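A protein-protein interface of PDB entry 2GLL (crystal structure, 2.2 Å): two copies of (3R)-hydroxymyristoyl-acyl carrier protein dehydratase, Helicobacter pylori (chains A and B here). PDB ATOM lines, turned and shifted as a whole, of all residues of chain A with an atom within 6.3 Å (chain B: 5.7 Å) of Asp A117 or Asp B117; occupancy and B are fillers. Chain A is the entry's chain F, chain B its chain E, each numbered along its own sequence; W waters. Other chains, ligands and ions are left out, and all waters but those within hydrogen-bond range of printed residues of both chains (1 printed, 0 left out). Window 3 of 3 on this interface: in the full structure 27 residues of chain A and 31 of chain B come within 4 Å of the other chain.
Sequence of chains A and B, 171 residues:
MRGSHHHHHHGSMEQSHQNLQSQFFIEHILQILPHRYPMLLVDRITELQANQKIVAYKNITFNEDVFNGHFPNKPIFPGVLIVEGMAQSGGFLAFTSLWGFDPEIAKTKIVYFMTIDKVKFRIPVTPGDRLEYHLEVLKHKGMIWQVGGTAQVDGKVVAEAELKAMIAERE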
ATOM      1  N   THR A 115      22.636   1.333  23.839  1.00  0.00           N
ATOM      2  CA  THR A 115      22.735   0.408  24.960  1.00  0.00           C
ATOM      3  C   THR A 115      21.757  -0.746  24.780  1.00  0.00           C
ATOM      4  O   THR A 115      20.757  -0.631  24.060  1.00  0.00           O
ATOM      5  CB  THR A 115      22.388   1.075  26.297  1.00  0.00           C
ATOM      6  OG1 THR A 115      21.012   1.466  26.278  1.00  0.00           O
ATOM      7  CG2 THR A 115      23.277   2.291  26.551  1.00  0.00           C
ATOM      8  N   ILE A 116      22.062  -1.858  25.441  1.00  0.00           N
ATOM      9  CA  ILE A 116      21.227  -3.057  25.420  1.00  0.00           C
ATOM     10  C   ILE A 116      21.344  -3.593  26.834  1.00  0.00           C
ATOM     11  O   ILE A 116      22.450  -3.652  27.380  1.00  0.00           O
ATOM     12  CB  ILE A 116      21.771  -4.152  24.482  1.00  0.00           C
ATOM     13  CG1 ILE A 116      21.977  -3.604  23.068  1.00  0.00           C
ATOM     14  CG2 ILE A 116      20.790  -5.319  24.453  1.00  0.00           C
ATOM     15  CD1 ILE A 116      22.747  -4.554  22.149  1.00  0.00           C
ATOM     16  N   ASP A 117      20.229  -3.977  27.439  1.00  0.00           N
ATOM     17  CA  ASP A 117      20.317  -4.484  28.798  1.00  0.00           C
ATOM     18  C   ASP A 117      19.168  -5.405  29.142  1.00  0.00           C
ATOM     19  O   ASP A 117      18.148  -5.438  28.450  1.00  0.00           O
ATOM     20  CB  ASP A 117      20.371  -3.315  29.790  1.00  0.00           C
ATOM     21  CG  ASP A 117      20.847  -3.734  31.182  1.00  0.00           C
ATOM     22  OD1 ASP A 117      21.333  -4.878  31.349  1.00  0.00           O
ATOM     23  OD2 ASP A 117      20.746  -2.903  32.108  1.00  0.00           O
ATOM     24  N   LYS A 118      19.369  -6.173  30.207  1.00  0.00           N
ATOM     25  CA  LYS A 118      18.372  -7.100  30.711  1.00  0.00           C
ATOM     26  C   LYS A 118      17.795  -8.049  29.665  1.00  0.00           C
ATOM     27  O   LYS A 118      16.578  -8.236  29.589  1.00  0.00           O
ATOM     28  CB  LYS A 118      17.248  -6.303  31.381  1.00  0.00           C
ATOM     29  CG  LYS A 118      17.762  -5.336  32.449  1.00  0.00           C
ATOM     30  CD  LYS A 118      16.638  -4.476  33.022  1.00  0.00           C
ATOM     31  CE  LYS A 118      17.170  -3.419  33.984  1.00  0.00           C
ATOM     32  NZ  LYS A 118      18.052  -2.429  33.278  1.00  0.00           N
ATOM     33  N   VAL A 119      18.651  -8.648  28.846  1.00  0.00           N
ATOM     34  CA  VAL A 119      18.132  -9.579  27.862  1.00  0.00           C
ATOM     35  C   VAL A 119      18.324 -11.013  28.339  1.00  0.00           C
ATOM     36  O   VAL A 119      19.369 -11.371  28.897  1.00  0.00           O
ATOM     37  CB  VAL A 119      18.768  -9.384  26.445  1.00  0.00           C
ATOM     38  CG1 VAL A 119      19.932  -8.420  26.500  1.00  0.00           C
ATOM     39  CG2 VAL A 119      19.202 -10.719  25.874  1.00  0.00           C
ATOM     40  N   GLU A 160      13.618 -11.698  26.136  1.00  0.00           N
ATOM     41  CA  GLU A 160      13.255 -10.429  26.760  1.00  0.00           C
ATOM     42  C   GLU A 160      14.423  -9.476  26.569  1.00  0.00           C
ATOM     43  O   GLU A 160      15.578  -9.913  26.545  1.00  0.00           O
ATOM     44  CB  GLU A 160      13.049 -10.622  28.258  1.00  0.00           C
ATOM     45  CG  GLU A 160      12.150 -11.786  28.608  1.00  0.00           C
ATOM     46  CD  GLU A 160      12.152 -12.084  30.088  1.00  0.00           C
ATOM     47  OE1 GLU A 160      11.649 -13.167  30.466  1.00  0.00           O
ATOM     48  OE2 GLU A 160      12.655 -11.239  30.866  1.00  0.00           O
ATOM     49  N   ALA A 161      14.144  -8.181  26.448  1.00  0.00           N
ATOM     50  CA  ALA A 161      15.228  -7.220  26.286  1.00  0.00           C
ATOM     51  C   ALA A 161      14.805  -5.763  26.403  1.00  0.00           C
ATOM     52  O   ALA A 161      13.624  -5.428  26.308  1.00  0.00           O
ATOM     53  CB  ALA A 161      15.928  -7.444  24.948  1.00  0.00           C
ATOM     54  N   GLU A 162      15.800  -4.909  26.616  1.00  0.00           N
ATOM     55  CA  GLU A 162      15.610  -3.467  26.723  1.00  0.00           C
ATOM     56  C   GLU A 162      16.761  -2.870  25.950  1.00  0.00           C
ATOM     57  O   GLU A 162      17.867  -3.410  25.972  1.00  0.00           O
ATOM     58  CB  GLU A 162      15.694  -2.998  28.172  1.00  0.00           C
ATOM     59  CG  GLU A 162      14.455  -3.253  29.008  1.00  0.00           C
ATOM     60  CD  GLU A 162      14.591  -2.646  30.395  1.00  0.00           C
ATOM     61  OE1 GLU A 162      15.504  -1.808  30.586  1.00  0.00           O
ATOM     62  OE2 GLU A 162      13.783  -2.996  31.287  1.00  0.00           O
ATOM     63  N   LEU A 163      16.524  -1.755  25.269  1.00  0.00           N
ATOM     64  CA  LEU A 163      17.592  -1.160  24.486  1.00  0.00           C
ATOM     65  C   LEU A 163      17.360   0.310  24.194  1.00  0.00           C
ATOM     66  O   LEU A 163      16.252   0.827  24.346  1.00  0.00           O
ATOM     67  CB  LEU A 163      17.754  -1.939  23.178  1.00  0.00           C
ATOM     68  CG  LEU A 163      16.537  -1.964  22.248  1.00  0.00           C
ATOM     69  CD1 LEU A 163      16.661  -0.843  21.229  1.00  0.00           C
ATOM     70  CD2 LEU A 163      16.451  -3.309  21.533  1.00  0.00           C
ATOM     71  N   THR B 115      22.134 -14.768  28.601  1.00  0.00           N
ATOM     72  CA  THR B 115      21.789 -13.384  28.932  1.00  0.00           C
ATOM     73  C   THR B 115      22.816 -12.385  28.402  1.00  0.00           C
ATOM     74  O   THR B 115      23.968 -12.728  28.120  1.00  0.00           O
ATOM     75  CB  THR B 115      21.698 -13.135  30.458  1.00  0.00           C
ATOM     76  OG1 THR B 115      22.993 -13.312  31.037  1.00  0.00           O
ATOM     77  CG2 THR B 115      20.699 -14.075  31.122  1.00  0.00           C
ATOM     78  N   ILE B 116      22.378 -11.137  28.285  1.00  0.00           N
ATOM     79  CA  ILE B 116      23.231 -10.051  27.833  1.00  0.00           C
ATOM     80  C   ILE B 116      22.850  -8.833  28.662  1.00  0.00           C
ATOM     81  O   ILE B 116      21.681  -8.454  28.703  1.00  0.00           O
ATOM     82  CB  ILE B 116      23.008  -9.740  26.345  1.00  0.00           C
ATOM     83  CG1 ILE B 116      23.323 -10.980  25.507  1.00  0.00           C
ATOM     84  CG2 ILE B 116      23.897  -8.584  25.914  1.00  0.00           C
ATOM     85  CD1 ILE B 116      23.176 -10.769  24.028  1.00  0.00           C
ATOM     86  N   ASP B 117      23.825  -8.229  29.336  1.00  0.00           N
ATOM     87  CA  ASP B 117      23.551  -7.058  30.159  1.00  0.00           C
ATOM     88  C   ASP B 117      24.565  -5.950  29.991  1.00  0.00           C
ATOM     89  O   ASP B 117      25.645  -6.146  29.426  1.00  0.00           O
ATOM     90  CB  ASP B 117      23.507  -7.418  31.648  1.00  0.00           C
ATOM     91  CG  ASP B 117      22.401  -8.384  31.984  1.00  0.00           C
ATOM     92  OD1 ASP B 117      22.609  -9.603  31.812  1.00  0.00           O
ATOM     93  OD2 ASP B 117      21.321  -7.926  32.418  1.00  0.00           O
ATOM     94  N   LYS B 118      24.185  -4.780  30.492  1.00  0.00           N
ATOM     95  CA  LYS B 118      25.020  -3.601  30.478  1.00  0.00           C
ATOM     96  C   LYS B 118      25.875  -3.406  29.239  1.00  0.00           C
ATOM     97  O   LYS B 118      27.078  -3.182  29.360  1.00  0.00           O
ATOM     98  CB  LYS B 118      25.934  -3.606  31.709  1.00  0.00           C
ATOM     99  CG  LYS B 118      25.252  -3.256  33.033  1.00  0.00           C
ATOM    100  CD  LYS B 118      24.184  -4.273  33.414  1.00  0.00           C
ATOM    101  CE  LYS B 118      23.617  -3.972  34.798  1.00  0.00           C
ATOM    102  NZ  LYS B 118      24.687  -3.991  35.852  1.00  0.00           N
ATOM    103  N   VAL B 119      25.292  -3.490  28.047  1.00  0.00           N
ATOM    104  CA  VAL B 119      26.110  -3.265  26.858  1.00  0.00           C
ATOM    105  C   VAL B 119      25.980  -1.801  26.471  1.00  0.00           C
ATOM    106  O   VAL B 119      24.927  -1.195  26.620  1.00  0.00           O
ATOM    107  CB  VAL B 119      25.706  -4.160  25.643  1.00  0.00           C
ATOM    108  CG1 VAL B 119      25.075  -5.442  26.123  1.00  0.00           C
ATOM    109  CG2 VAL B 119      24.801  -3.405  24.701  1.00  0.00           C
ATOM    110  N   GLU B 160      31.044  -2.008  25.367  1.00  0.00           N
ATOM    111  CA  GLU B 160      31.147  -2.687  26.656  1.00  0.00           C
ATOM    112  C   GLU B 160      30.012  -3.696  26.696  1.00  0.00           C
ATOM    113  O   GLU B 160      28.936  -3.440  26.154  1.00  0.00           O
ATOM    114  CB  GLU B 160      30.942  -1.712  27.820  1.00  0.00           C
ATOM    115  CG  GLU B 160      31.820  -0.473  27.809  1.00  0.00           C
ATOM    116  CD  GLU B 160      31.239   0.619  28.681  1.00  0.00           C
ATOM    117  OE1 GLU B 160      31.813   1.725  28.718  1.00  0.00           O
ATOM    118  OE2 GLU B 160      30.207   0.372  29.340  1.00  0.00           O
ATOM    119  N   ALA B 161      30.246  -4.831  27.342  1.00  0.00           N
ATOM    120  CA  ALA B 161      29.213  -5.847  27.444  1.00  0.00           C
ATOM    121  C   ALA B 161      29.495  -6.899  28.507  1.00  0.00           C
ATOM    122  O   ALA B 161      30.644  -7.226  28.815  1.00  0.00           O
ATOM    123  CB  ALA B 161      29.010  -6.530  26.087  1.00  0.00           C
ATOM    124  N   GLU B 162      28.414  -7.424  29.060  1.00  0.00           N
ATOM    125  CA  GLU B 162      28.472  -8.473  30.061  1.00  0.00           C
ATOM    126  C   GLU B 162      27.529  -9.528  29.493  1.00  0.00           C
ATOM    127  O   GLU B 162      26.426  -9.195  29.060  1.00  0.00           O
ATOM    128  CB  GLU B 162      27.936  -7.949  31.386  1.00  0.00           C
ATOM    129  CG  GLU B 162      27.909  -8.971  32.492  1.00  0.00           C
ATOM    130  CD  GLU B 162      27.145  -8.468  33.694  1.00  0.00           C
ATOM    131  OE1 GLU B 162      27.506  -7.386  34.209  1.00  0.00           O
ATOM    132  OE2 GLU B 162      26.181  -9.155  34.109  1.00  0.00           O
ATOM    133  N   LEU B 163      27.950 -10.786  29.475  1.00  0.00           N
ATOM    134  CA  LEU B 163      27.087 -11.832  28.931  1.00  0.00           C
ATOM    135  C   LEU B 163      27.315 -13.195  29.567  1.00  0.00           C
ATOM    136  O   LEU B 163      28.412 -13.502  30.042  1.00  0.00           O
ATOM    137  CB  LEU B 163      27.278 -11.935  27.412  1.00  0.00           C
ATOM    138  CG  LEU B 163      28.601 -12.538  26.938  1.00  0.00           C
ATOM    139  CD1 LEU B 163      28.390 -14.022  26.646  1.00  0.00           C
ATOM    140  CD2 LEU B 163      29.094 -11.820  25.678  1.00  0.00           C
HETATM  141  O   HOH W   1      19.834 -10.077  31.810  1.00  0.00           O
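Of chain B, only Ile B116 (3.98 Å), Asp B117 (3.2 Å) and Lys B118 (3.0 Å) come within 4 Å of Asp A117.
Of the printed residues of chain B, Lys A118 touches Ile B116 (3.6 Å) and Asp B117 (3.4 Å).
Of the printed residues of chain A, Thr B115 touches Val A119.
Of the printed residues of chain A, Ile B116 touches Asp A117, Lys A118 and Val A119.
Printed residues of chain A within 4 Å of Asp B117: Asp A117 and Lys A118.
The nearest residue of chain A that does not touch Asp B117 is Ile A116 (4.1 Å).
Ile A116 touches Lys B118, and with the chains exchanged Lys A118 touches Ile B116.
Ile A116 touches Val B119, and with the chains exchanged Val A119 touches Ile B116.
Asp A117 touches Ile B116, but with the chains exchanged Ile A116 does not touch Asp B117 (4.1 Å).
Asp B117 touches its own counterpart, Asp A117.
Positions printed for both chains: 115, 116, 117, 118, 119, 160, 161, 162 and 163.
Of the 10 pairs that touch across the chains among the printed residues, 9 have their exchanged pair printed and touching as well.
Water W1 lies within hydrogen-bond range of OD2 of Asp B117 and O of Val A119.
Among the printed residues, pairs that only touch across the chains: Val A119 with Thr B115, Thr A115 with Val B119, Lys A118 with Ile B116, Ile A116 with Lys B118 and Asp A117 with Ile B116.
N of Asp B117 sits at hydrogen-bond distance from O of Glu B162, at 2.8 Å.
NZ of Lys A118 lies within salt-bridge range of OD2 of Asp A117 (3.0 Å).
N of Asp A117 is in hydrogen-bond range of O of Glu A162.
OE1 of Glu A162 is in salt-bridge range of NZ of Lys A118, at 3.8 Å.
The backbone carbonyl oxygen of Ile B116 lies close to the backbone NH of Val A119 (3.0 Å).
The side-chain carboxylate (OD2) of Asp B117 sits at hydrogen-bond distance from the backbone NH (N) of Lys A118 (3.4 Å).
The backbone NH (N) of Lys B118 sits at hydrogen-bond distance from the side-chain carboxylate (OD1) of Asp A117 (3.0 Å).
N of Val B119 lies within hydrogen-bond range of O of Ile A116, at 2.9 Å.
The side-chain carboxylate (OD2) of Asp B117 lies close to the side-chain carboxylate (OD1) of Asp A117 (3.2 Å).
Of the 9 printed residues of chain A, 5 touch a printed residue of chain B.
Hydrophobic or aromatic side chains of chain A within 4 Å of the printed part of chain B: Ile A116 and Val A119.
Hydrophobic or aromatic side chains of chain B that line the printed part of chain A: Ile B116 and Val B119.
Among the printed residues, 10 pairs touch across the chains.
Among the printed residues, no Asp or Glu carboxylate lies within 4 Å of a Lys or Arg side-chain nitrogen of the other chain.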
